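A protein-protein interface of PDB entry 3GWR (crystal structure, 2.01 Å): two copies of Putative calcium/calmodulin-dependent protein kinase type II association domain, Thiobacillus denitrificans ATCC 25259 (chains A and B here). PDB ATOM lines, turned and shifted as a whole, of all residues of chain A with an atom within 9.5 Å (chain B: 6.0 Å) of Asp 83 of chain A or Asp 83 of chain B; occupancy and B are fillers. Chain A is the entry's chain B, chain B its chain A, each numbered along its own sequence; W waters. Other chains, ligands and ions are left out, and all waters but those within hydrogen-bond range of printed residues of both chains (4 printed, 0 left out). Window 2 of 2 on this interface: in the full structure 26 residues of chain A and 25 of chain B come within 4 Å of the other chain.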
ATOM      1  N   PRO A  10      24.281 -21.729  -6.951  1.00  0.00           N
ATOM      2  CA  PRO A  10      25.730 -21.591  -6.760  1.00  0.00           C
ATOM      3  C   PRO A  10      26.464 -21.187  -8.043  1.00  0.00           C
ATOM      4  O   PRO A  10      27.397 -20.421  -7.994  1.00  0.00           O
ATOM      5  CB  PRO A  10      26.170 -22.997  -6.324  1.00  0.00           C
ATOM      6  CG  PRO A  10      24.996 -23.790  -6.276  1.00  0.00           C
ATOM      7  CD  PRO A  10      23.795 -23.052  -6.599  1.00  0.00           C
ATOM      8  N   ILE A  79      31.589 -30.502  -5.369  1.00  0.00           N
ATOM      9  CA  ILE A  79      30.997 -31.332  -4.337  1.00  0.00           C
ATOM     10  C   ILE A  79      29.676 -30.642  -4.003  1.00  0.00           C
ATOM     11  O   ILE A  79      29.649 -29.552  -3.419  1.00  0.00           O
ATOM     12  CB  ILE A  79      31.840 -31.445  -3.070  1.00  0.00           C
ATOM     13  CG1 ILE A  79      33.242 -31.960  -3.422  1.00  0.00           C
ATOM     14  CG2 ILE A  79      31.152 -32.407  -2.054  1.00  0.00           C
ATOM     15  CD1 ILE A  79      34.224 -31.833  -2.275  1.00  0.00           C
ATOM     16  N   ARG A  80      28.588 -31.311  -4.349  1.00  0.00           N
ATOM     17  CA  ARG A  80      27.264 -30.755  -4.234  1.00  0.00           C
ATOM     18  C   ARG A  80      26.426 -31.353  -3.106  1.00  0.00           C
ATOM     19  O   ARG A  80      26.266 -32.566  -3.030  1.00  0.00           O
ATOM     20  CB  ARG A  80      26.586 -30.976  -5.583  1.00  0.00           C
ATOM     21  CG  ARG A  80      25.184 -30.441  -5.743  1.00  0.00           C
ATOM     22  CD  ARG A  80      24.786 -30.528  -7.219  1.00  0.00           C
ATOM     23  NE  ARG A  80      25.399 -29.432  -7.931  1.00  0.00           N
ATOM     24  CZ  ARG A  80      24.781 -28.300  -8.263  1.00  0.00           C
ATOM     25  NH1 ARG A  80      23.493 -28.107  -8.020  1.00  0.00           N
ATOM     26  NH2 ARG A  80      25.451 -27.358  -8.893  1.00  0.00           N
ATOM     27  N   GLN A  81      25.983 -30.500  -2.174  1.00  0.00           N
ATOM     28  CA  GLN A  81      24.995 -30.890  -1.160  1.00  0.00           C
ATOM     29  C   GLN A  81      23.853 -29.882  -1.207  1.00  0.00           C
ATOM     30  O   GLN A  81      23.922 -28.878  -1.925  1.00  0.00           O
ATOM     31  CB  GLN A  81      25.624 -31.054   0.236  1.00  0.00           C
ATOM     32  CG  GLN A  81      26.696 -32.188   0.275  1.00  0.00           C
ATOM     33  CD  GLN A  81      26.113 -33.619   0.135  1.00  0.00           C
ATOM     34  OE1 GLN A  81      24.910 -33.832   0.229  1.00  0.00           O
ATOM     35  NE2 GLN A  81      27.000 -34.600  -0.064  1.00  0.00           N
ATOM     36  N   ALA A  82      22.782 -30.150  -0.483  1.00  0.00           N
ATOM     37  CA  ALA A  82      21.614 -29.278  -0.588  1.00  0.00           C
ATOM     38  C   ALA A  82      21.908 -27.888  -0.015  1.00  0.00           C
ATOM     39  O   ALA A  82      21.486 -26.896  -0.584  1.00  0.00           O
ATOM     40  CB  ALA A  82      20.370 -29.913   0.133  1.00  0.00           C
ATOM     41  N   ASP A  83      22.662 -27.839   1.085  1.00  0.00           N
ATOM     42  CA  ASP A  83      22.925 -26.583   1.824  1.00  0.00           C
ATOM     43  C   ASP A  83      24.245 -25.854   1.492  1.00  0.00           C
ATOM     44  O   ASP A  83      24.383 -24.658   1.748  1.00  0.00           O
ATOM     45  CB  ASP A  83      22.904 -26.887   3.322  1.00  0.00           C
ATOM     46  CG  ASP A  83      23.985 -27.859   3.725  1.00  0.00           C
ATOM     47  OD1 ASP A  83      24.046 -28.950   3.122  1.00  0.00           O
ATOM     48  OD2 ASP A  83      24.781 -27.522   4.610  1.00  0.00           O
ATOM     49  N   HIS A  84      25.228 -26.608   0.996  1.00  0.00           N
ATOM     50  CA  HIS A  84      26.529 -26.094   0.610  1.00  0.00           C
ATOM     51  C   HIS A  84      27.012 -26.765  -0.661  1.00  0.00           C
ATOM     52  O   HIS A  84      26.898 -27.990  -0.814  1.00  0.00           O
ATOM     53  CB  HIS A  84      27.598 -26.311   1.704  1.00  0.00           C
ATOM     54  CG  HIS A  84      27.534 -25.331   2.853  1.00  0.00           C
ATOM     55  ND1 HIS A  84      26.664 -25.470   3.920  1.00  0.00           N
ATOM     56  CD2 HIS A  84      28.297 -24.244   3.136  1.00  0.00           C
ATOM     57  CE1 HIS A  84      26.861 -24.483   4.777  1.00  0.00           C
ATOM     58  NE2 HIS A  84      27.840 -23.722   4.322  1.00  0.00           N
ATOM     59  N   VAL A  85      27.613 -25.969  -1.534  1.00  0.00           N
ATOM     60  CA  VAL A  85      28.166 -26.462  -2.798  1.00  0.00           C
ATOM     61  C   VAL A  85      29.599 -25.952  -2.900  1.00  0.00           C
ATOM     62  O   VAL A  85      29.827 -24.761  -2.710  1.00  0.00           O
ATOM     63  CB  VAL A  85      27.316 -26.069  -3.996  1.00  0.00           C
ATOM     64  CG1 VAL A  85      28.077 -26.365  -5.331  1.00  0.00           C
ATOM     65  CG2 VAL A  85      25.990 -26.824  -3.957  1.00  0.00           C
ATOM     66  N   ILE A  86      30.558 -26.883  -3.066  1.00  0.00           N
ATOM     67  CA  ILE A  86      31.975 -26.558  -3.218  1.00  0.00           C
ATOM     68  C   ILE A  86      32.337 -26.739  -4.681  1.00  0.00           C
ATOM     69  O   ILE A  86      32.020 -27.772  -5.259  1.00  0.00           O
ATOM     70  CB  ILE A  86      32.850 -27.497  -2.378  1.00  0.00           C
ATOM     71  CG1 ILE A  86      32.443 -27.382  -0.910  1.00  0.00           C
ATOM     72  CG2 ILE A  86      34.323 -27.139  -2.598  1.00  0.00           C
ATOM     73  CD1 ILE A  86      33.037 -28.520  -0.019  1.00  0.00           C
ATOM     74  N   VAL A 110      33.360 -21.984  -1.867  1.00  0.00           N
ATOM     75  CA  VAL A 110      32.283 -22.607  -1.117  1.00  0.00           C
ATOM     76  C   VAL A 110      31.100 -21.654  -1.073  1.00  0.00           C
ATOM     77  O   VAL A 110      31.250 -20.509  -0.619  1.00  0.00           O
ATOM     78  CB  VAL A 110      32.707 -22.932   0.351  1.00  0.00           C
ATOM     79  CG1 VAL A 110      31.541 -23.576   1.094  1.00  0.00           C
ATOM     80  CG2 VAL A 110      33.986 -23.823   0.397  1.00  0.00           C
ATOM     81  N   TYR A 111      29.942 -22.151  -1.539  1.00  0.00           N
ATOM     82  CA  TYR A 111      28.668 -21.425  -1.595  1.00  0.00           C
ATOM     83  C   TYR A 111      27.683 -22.031  -0.612  1.00  0.00           C
ATOM     84  O   TYR A 111      27.589 -23.262  -0.477  1.00  0.00           O
ATOM     85  CB  TYR A 111      28.087 -21.480  -3.011  1.00  0.00           C
ATOM     86  CG  TYR A 111      29.075 -20.935  -4.004  1.00  0.00           C
ATOM     87  CD1 TYR A 111      29.222 -19.542  -4.184  1.00  0.00           C
ATOM     88  CD2 TYR A 111      29.939 -21.785  -4.709  1.00  0.00           C
ATOM     89  CE1 TYR A 111      30.177 -19.031  -5.066  1.00  0.00           C
ATOM     90  CE2 TYR A 111      30.896 -21.279  -5.605  1.00  0.00           C
ATOM     91  CZ  TYR A 111      31.024 -19.893  -5.765  1.00  0.00           C
ATOM     92  OH  TYR A 111      31.988 -19.386  -6.655  1.00  0.00           O
ATOM     93  N   ARG A 112      26.985 -21.148   0.086  1.00  0.00           N
ATOM     94  CA  ARG A 112      26.027 -21.507   1.114  1.00  0.00           C
ATOM     95  C   ARG A 112      24.641 -21.035   0.712  1.00  0.00           C
ATOM     96  O   ARG A 112      24.459 -19.911   0.269  1.00  0.00           O
ATOM     97  CB  ARG A 112      26.369 -20.813   2.416  1.00  0.00           C
ATOM     98  CG  ARG A 112      25.324 -21.051   3.515  1.00  0.00           C
ATOM     99  CD  ARG A 112      25.373 -19.917   4.567  1.00  0.00           C
ATOM    100  NE  ARG A 112      26.568 -20.037   5.357  1.00  0.00           N
ATOM    101  CZ  ARG A 112      27.014 -19.129   6.224  1.00  0.00           C
ATOM    102  NH1 ARG A 112      26.400 -17.958   6.402  1.00  0.00           N
ATOM    103  NH2 ARG A 112      28.123 -19.407   6.898  1.00  0.00           N
ATOM    104  N   ARG A 113      23.663 -21.901   0.907  1.00  0.00           N
ATOM    105  CA  ARG A 113      22.283 -21.611   0.569  1.00  0.00           C
ATOM    106  C   ARG A 113      21.673 -20.759   1.633  1.00  0.00           C
ATOM    107  O   ARG A 113      21.957 -20.951   2.811  1.00  0.00           O
ATOM    108  CB  ARG A 113      21.514 -22.928   0.533  1.00  0.00           C
ATOM    109  CG  ARG A 113      20.092 -22.880   0.064  1.00  0.00           C
ATOM    110  CD  ARG A 113      19.355 -24.185   0.401  1.00  0.00           C
ATOM    111  NE  ARG A 113      19.375 -24.415   1.855  1.00  0.00           N
ATOM    112  CZ  ARG A 113      19.299 -25.608   2.444  1.00  0.00           C
ATOM    113  NH1 ARG A 113      19.162 -26.709   1.727  1.00  0.00           N
ATOM    114  NH2 ARG A 113      19.408 -25.716   3.762  1.00  0.00           N
ATOM    115  N   GLU A 114      20.787 -19.871   1.226  1.00  0.00           N
ATOM    116  CA  GLU A 114      20.013 -19.028   2.157  1.00  0.00           C
ATOM    117  C   GLU A 114      18.582 -19.201   1.701  1.00  0.00           C
ATOM    118  O   GLU A 114      18.353 -19.830   0.645  1.00  0.00           O
ATOM    119  CB  GLU A 114      20.451 -17.574   2.114  1.00  0.00           C
ATOM    120  CG  GLU A 114      21.956 -17.405   2.134  1.00  0.00           C
ATOM    121  CD  GLU A 114      22.395 -15.937   2.210  1.00  0.00           C
ATOM    122  OE1 GLU A 114      21.697 -15.078   1.607  1.00  0.00           O
ATOM    123  OE2 GLU A 114      23.439 -15.661   2.864  1.00  0.00           O
ATOM    124  N   ALA A 115      17.622 -18.669   2.453  1.00  0.00           N
ATOM    125  CA  ALA A 115      16.205 -18.855   2.088  1.00  0.00           C
ATOM    126  C   ALA A 115      15.823 -18.370   0.683  1.00  0.00           C
ATOM    127  O   ALA A 115      14.857 -18.895   0.053  1.00  0.00           O
ATOM    128  CB  ALA A 115      15.260 -18.209   3.135  1.00  0.00           C
ATOM    129  N   GLY A 117      18.395 -17.421  -1.855  1.00  0.00           N
ATOM    130  CA  GLY A 117      19.459 -17.554  -2.845  1.00  0.00           C
ATOM    131  C   GLY A 117      20.765 -18.107  -2.269  1.00  0.00           C
ATOM    132  O   GLY A 117      20.764 -18.715  -1.201  1.00  0.00           O
ATOM    133  N   TRP A 118      21.866 -17.883  -2.973  1.00  0.00           N
ATOM    134  CA  TRP A 118      23.208 -18.389  -2.567  1.00  0.00           C
ATOM    135  C   TRP A 118      24.247 -17.285  -2.471  1.00  0.00           C
ATOM    136  O   TRP A 118      24.152 -16.322  -3.199  1.00  0.00           O
ATOM    137  CB  TRP A 118      23.733 -19.491  -3.577  1.00  0.00           C
ATOM    138  CG  TRP A 118      22.874 -20.690  -3.634  1.00  0.00           C
ATOM    139  CD1 TRP A 118      21.623 -20.796  -4.198  1.00  0.00           C
ATOM    140  CD2 TRP A 118      23.194 -21.988  -3.132  1.00  0.00           C
ATOM    141  NE1 TRP A 118      21.143 -22.065  -4.037  1.00  0.00           N
ATOM    142  CE2 TRP A 118      22.088 -22.817  -3.386  1.00  0.00           C
ATOM    143  CE3 TRP A 118      24.287 -22.513  -2.437  1.00  0.00           C
ATOM    144  CZ2 TRP A 118      22.068 -24.164  -3.010  1.00  0.00           C
ATOM    145  CZ3 TRP A 118      24.266 -23.855  -2.077  1.00  0.00           C
ATOM    146  CH2 TRP A 118      23.161 -24.647  -2.331  1.00  0.00           C
ATOM    147  N   ARG A 119      25.193 -17.453  -1.529  1.00  0.00           N
ATOM    148  CA  ARG A 119      26.294 -16.522  -1.322  1.00  0.00           C
ATOM    149  C   ARG A 119      27.578 -17.282  -1.040  1.00  0.00           C
ATOM    150  O   ARG A 119      27.552 -18.390  -0.572  1.00  0.00           O
ATOM    151  CB  ARG A 119      26.018 -15.601  -0.134  1.00  0.00           C
ATOM    152  CG  ARG A 119      24.922 -14.576  -0.345  1.00  0.00           C
ATOM    153  CD  ARG A 119      25.359 -13.468  -1.287  1.00  0.00           C
ATOM    154  NE  ARG A 119      24.320 -12.455  -1.458  1.00  0.00           N
ATOM    155  CZ  ARG A 119      24.291 -11.242  -0.900  1.00  0.00           C
ATOM    156  NH1 ARG A 119      25.259 -10.780  -0.101  1.00  0.00           N
ATOM    157  NH2 ARG A 119      23.259 -10.454  -1.181  1.00  0.00           N
ATOM    158  N   VAL A 121      30.893 -18.093   1.039  1.00  0.00           N
ATOM    159  CA  VAL A 121      31.413 -18.005   2.416  1.00  0.00           C
ATOM    160  C   VAL A 121      32.948 -18.203   2.494  1.00  0.00           C
ATOM    161  O   VAL A 121      33.586 -17.848   3.489  1.00  0.00           O
ATOM    162  CB  VAL A 121      30.713 -18.996   3.393  1.00  0.00           C
ATOM    163  CG1 VAL A 121      29.152 -18.639   3.528  1.00  0.00           C
ATOM    164  CG2 VAL A 121      30.975 -20.480   3.000  1.00  0.00           C
ATOM    165  N   GLN B  81      27.998 -24.135  10.680  1.00  0.00           N
ATOM    166  CA  GLN B  81      26.607 -24.220  10.255  1.00  0.00           C
ATOM    167  C   GLN B  81      26.080 -25.608  10.636  1.00  0.00           C
ATOM    168  O   GLN B  81      26.862 -26.501  11.069  1.00  0.00           O
ATOM    169  CB  GLN B  81      26.481 -23.927   8.771  1.00  0.00           C
ATOM    170  CG  GLN B  81      26.832 -22.471   8.399  1.00  0.00           C
ATOM    171  CD  GLN B  81      25.759 -21.498   8.794  1.00  0.00           C
ATOM    172  OE1 GLN B  81      24.583 -21.731   8.554  1.00  0.00           O
ATOM    173  NE2 GLN B  81      26.161 -20.398   9.434  1.00  0.00           N
ATOM    174  N   ALA B  82      24.772 -25.792  10.481  1.00  0.00           N
ATOM    175  CA  ALA B  82      24.113 -27.012  10.942  1.00  0.00           C
ATOM    176  C   ALA B  82      24.644 -28.324  10.356  1.00  0.00           C
ATOM    177  O   ALA B  82      24.901 -29.256  11.117  1.00  0.00           O
ATOM    178  CB  ALA B  82      22.623 -26.904  10.784  1.00  0.00           C
ATOM    179  N   ASP B  83      24.911 -28.352   9.044  1.00  0.00           N
ATOM    180  CA  ASP B  83      25.299 -29.565   8.315  1.00  0.00           C
ATOM    181  C   ASP B  83      26.676 -29.543   7.704  1.00  0.00           C
ATOM    182  O   ASP B  83      27.097 -30.569   7.160  1.00  0.00           O
ATOM    183  CB  ASP B  83      24.294 -29.833   7.179  1.00  0.00           C
ATOM    184  CG  ASP B  83      22.904 -30.105   7.678  1.00  0.00           C
ATOM    185  OD1 ASP B  83      22.738 -30.437   8.870  1.00  0.00           O
ATOM    186  OD2 ASP B  83      21.966 -29.988   6.860  1.00  0.00           O
ATOM    187  N   HIS B  84      27.342 -28.389   7.726  1.00  0.00           N
ATOM    188  CA  HIS B  84      28.743 -28.270   7.308  1.00  0.00           C
ATOM    189  C   HIS B  84      29.475 -27.300   8.248  1.00  0.00           C
ATOM    190  O   HIS B  84      28.936 -26.233   8.610  1.00  0.00           O
ATOM    191  CB  HIS B  84      28.896 -27.799   5.870  1.00  0.00           C
ATOM    192  CG  HIS B  84      28.474 -28.805   4.841  1.00  0.00           C
ATOM    193  ND1 HIS B  84      27.166 -28.948   4.438  1.00  0.00           N
ATOM    194  CD2 HIS B  84      29.193 -29.692   4.108  1.00  0.00           C
ATOM    195  CE1 HIS B  84      27.085 -29.905   3.529  1.00  0.00           C
ATOM    196  NE2 HIS B  84      28.302 -30.374   3.309  1.00  0.00           N
ATOM    197  N   VAL B  85      30.692 -27.686   8.618  1.00  0.00           N
ATOM    198  CA  VAL B  85      31.581 -26.876   9.454  1.00  0.00           C
ATOM    199  C   VAL B  85      32.955 -26.788   8.766  1.00  0.00           C
ATOM    200  O   VAL B  85      33.498 -27.803   8.316  1.00  0.00           O
ATOM    201  CB  VAL B  85      31.697 -27.447  10.858  1.00  0.00           C
ATOM    202  CG1 VAL B  85      32.895 -26.828  11.637  1.00  0.00           C
ATOM    203  CG2 VAL B  85      30.353 -27.304  11.606  1.00  0.00           C
ATOM    204  N   TYR B 111      33.929 -30.371   7.168  1.00  0.00           N
ATOM    205  CA  TYR B 111      33.211 -31.522   7.714  1.00  0.00           C
ATOM    206  C   TYR B 111      31.710 -31.451   7.413  1.00  0.00           C
ATOM    207  O   TYR B 111      31.082 -30.381   7.513  1.00  0.00           O
ATOM    208  CB  TYR B 111      33.455 -31.604   9.227  1.00  0.00           C
ATOM    209  CG  TYR B 111      34.938 -31.577   9.534  1.00  0.00           C
ATOM    210  CD1 TYR B 111      35.670 -32.772   9.682  1.00  0.00           C
ATOM    211  CD2 TYR B 111      35.631 -30.368   9.593  1.00  0.00           C
ATOM    212  CE1 TYR B 111      37.011 -32.747   9.905  1.00  0.00           C
ATOM    213  CE2 TYR B 111      36.987 -30.333   9.848  1.00  0.00           C
ATOM    214  CZ  TYR B 111      37.678 -31.533   9.982  1.00  0.00           C
ATOM    215  OH  TYR B 111      39.013 -31.525  10.227  1.00  0.00           O
ATOM    216  N   ARG B 112      31.142 -32.603   7.052  1.00  0.00           N
ATOM    217  CA  ARG B 112      29.715 -32.731   6.757  1.00  0.00           C
ATOM    218  C   ARG B 112      29.060 -33.542   7.864  1.00  0.00           C
ATOM    219  O   ARG B 112      29.617 -34.548   8.287  1.00  0.00           O
ATOM    220  CB  ARG B 112      29.564 -33.511   5.474  1.00  0.00           C
ATOM    221  CG  ARG B 112      28.227 -33.532   4.884  1.00  0.00           C
ATOM    222  CD  ARG B 112      28.236 -34.391   3.597  1.00  0.00           C
ATOM    223  NE  ARG B 112      28.279 -35.806   3.933  1.00  0.00           N
ATOM    224  CZ  ARG B 112      28.632 -36.792   3.110  1.00  0.00           C
ATOM    225  NH1 ARG B 112      29.018 -36.540   1.863  1.00  0.00           N
ATOM    226  NH2 ARG B 112      28.620 -38.047   3.559  1.00  0.00           N
ATOM    227  N   ARG B 113      27.865 -33.134   8.280  1.00  0.00           N
ATOM    228  CA  ARG B 113      27.121 -33.867   9.294  1.00  0.00           C
ATOM    229  C   ARG B 113      26.355 -35.030   8.644  1.00  0.00           C
ATOM    230  O   ARG B 113      25.687 -34.852   7.642  1.00  0.00           O
ATOM    231  CB  ARG B 113      26.148 -32.941  10.026  1.00  0.00           C
ATOM    232  CG  ARG B 113      25.469 -33.568  11.246  1.00  0.00           C
ATOM    233  CD  ARG B 113      24.620 -32.545  11.966  1.00  0.00           C
ATOM    234  NE  ARG B 113      23.457 -32.149  11.164  1.00  0.00           N
ATOM    235  CZ  ARG B 113      22.283 -32.780  11.164  1.00  0.00           C
ATOM    236  NH1 ARG B 113      22.083 -33.830  11.937  1.00  0.00           N
ATOM    237  NH2 ARG B 113      21.293 -32.349  10.387  1.00  0.00           N
ATOM    238  N   TRP B 118      30.073 -36.851  12.165  1.00  0.00           N
ATOM    239  CA  TRP B 118      30.659 -36.002  11.144  1.00  0.00           C
ATOM    240  C   TRP B 118      31.794 -36.688  10.410  1.00  0.00           C
ATOM    241  O   TRP B 118      32.494 -37.506  10.983  1.00  0.00           O
ATOM    242  CB  TRP B 118      31.201 -34.743  11.810  1.00  0.00           C
ATOM    243  CG  TRP B 118      30.130 -33.890  12.431  1.00  0.00           C
ATOM    244  CD1 TRP B 118      29.475 -34.137  13.602  1.00  0.00           C
ATOM    245  CD2 TRP B 118      29.608 -32.653  11.933  1.00  0.00           C
ATOM    246  NE1 TRP B 118      28.565 -33.144  13.845  1.00  0.00           N
ATOM    247  CE2 TRP B 118      28.627 -32.221  12.842  1.00  0.00           C
ATOM    248  CE3 TRP B 118      29.844 -31.883  10.788  1.00  0.00           C
ATOM    249  CZ2 TRP B 118      27.907 -31.052  12.654  1.00  0.00           C
ATOM    250  CZ3 TRP B 118      29.131 -30.730  10.611  1.00  0.00           C
ATOM    251  CH2 TRP B 118      28.174 -30.325  11.536  1.00  0.00           C
HETATM  252  O   HOH W   1      28.522 -19.000   9.971  1.00  0.00           O
HETATM  253  O   HOH W   2      21.829 -30.361   4.058  1.00  0.00           O
HETATM  254  O   HOH W   3      29.689 -34.066   0.440  1.00  0.00           O
HETATM  255  O   HOH W   4      24.030 -26.345   6.978  1.00  0.00           O
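The side-chain amide nitrogen (NE2) of Gln 81 of chain B lies close to the guanidinium group (NH2) of Arg 112 of chain A. A ring nitrogen (ND1) of His 84 of chain B lies within hydrogen-bond range of the side-chain carboxylate (OD2) of Asp 83 of chain A, at 2.8 Å. NE2 of Gln 81 of chain A sits close to NH1 of Arg 112 of chain B, at 3.4 Å.
The side-chain carboxylate (OD1) of Asp 83 of chain B is in salt-bridge range of the guanidinium group (NH2) of Arg 113 of chain B. The side-chain carboxylate (OD2) of Asp 83 of chain A is in hydrogen-bond range of a ring nitrogen (ND1) of His 84 of chain A (2.9 Å). The backbone carbonyl oxygen (O) of Asp 83 of chain A lies within hydrogen-bond range of the backbone NH (N) of Arg 113 of chain A (3.0 Å). The backbone carbonyl oxygen (O) of Arg 119 of chain A sits at hydrogen-bond distance from the backbone NH (N) of Arg 112 of chain A, at 2.9 Å.
Gln 81 of chain A touches His 84 of chain B. Asp 83 of chain A touches Asp 83 of chain B. ND1 of His 84 of chain B touches ND1 of His 84 of chain A, 3.6 Å away.
Printed residues of chain B within 4 Å of Gln 81 of chain A: His 84 and Arg 112. Asp 83 of chain A touches just these residues of chain B: Asp 83 and His 84. Of the printed residues of chain B, Arg 112 of chain A touches Gln 81 (3.4 Å). Of the printed residues of chain A, Gln 81 of chain B touches Arg 112. No residue of chain A comes within 4 Å of Ala 82 of chain B. Printed residues of chain A within 4 Å of Arg 112 of chain B: Gln 81. No residue of chain A comes within 4 Å of Arg 113 of chain B. The nearest residue of chain B that does not touch Asp 83 of chain A is Gln 81 of chain B (5.8 Å). The nearest residue of chain A that does not touch Asp 83 of chain B is His 84 of chain A (5.6 Å). The nearest printed residue of chain B that does not touch Arg 112 of chain A is His 84 of chain B (7.1 Å).
Of the 19 printed residues of chain A, 4 touch a printed residue of chain B. Hydrophobic or aromatic side chains of chain A that line the printed part of chain B: His 84. Hydrophobic or aromatic side chains of chain B within 4 Å of the printed part of chain A: His 84. Among the printed residues, 6 pairs touch across the chains. Among the printed residues, no Asp or Glu carboxylate lies within 4 Å of a Lys or Arg side-chain nitrogen of the other chain.
Gln 81 of chain A touches His 84 of chain B, but with the chains exchanged His 84 of chain A does not touch Gln 81 of chain B (4.1 Å). Gln 81 of chain A touches Arg 112 of chain B, and with the chains exchanged Arg 112 of chain A touches Gln 81 of chain B. Asp 83 of chain A touches His 84 of chain B, but with the chains exchanged His 84 of chain A does not touch Asp 83 of chain B (5.6 Å). His 84 of chain A touches its own counterpart, His 84 of chain B. Positions printed for both chains: 81, 82, 83, 84, 85, 111, 112, 113 and 118.
Water W4 bridges OD2 of Asp 83 of chain A (2.7 Å) and N of Asp 83 of chain B (3.0 Å). Water W3 bridges the side-chain amide nitrogen (NE2) of Gln 81 of chain A (2.8 Å) and the guanidinium group (NH1) of Arg 112 of chain B (2.9 Å). Water W2 lies within hydrogen-bond range of OD1 of Asp 83 of chain A (2.8 Å) and OD2 of Asp 83 of chain B (2.8 Å). Water W1 lies within hydrogen-bond range of NE2 of Gln 81 of chain B and NH2 of Arg 112 of chain A.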
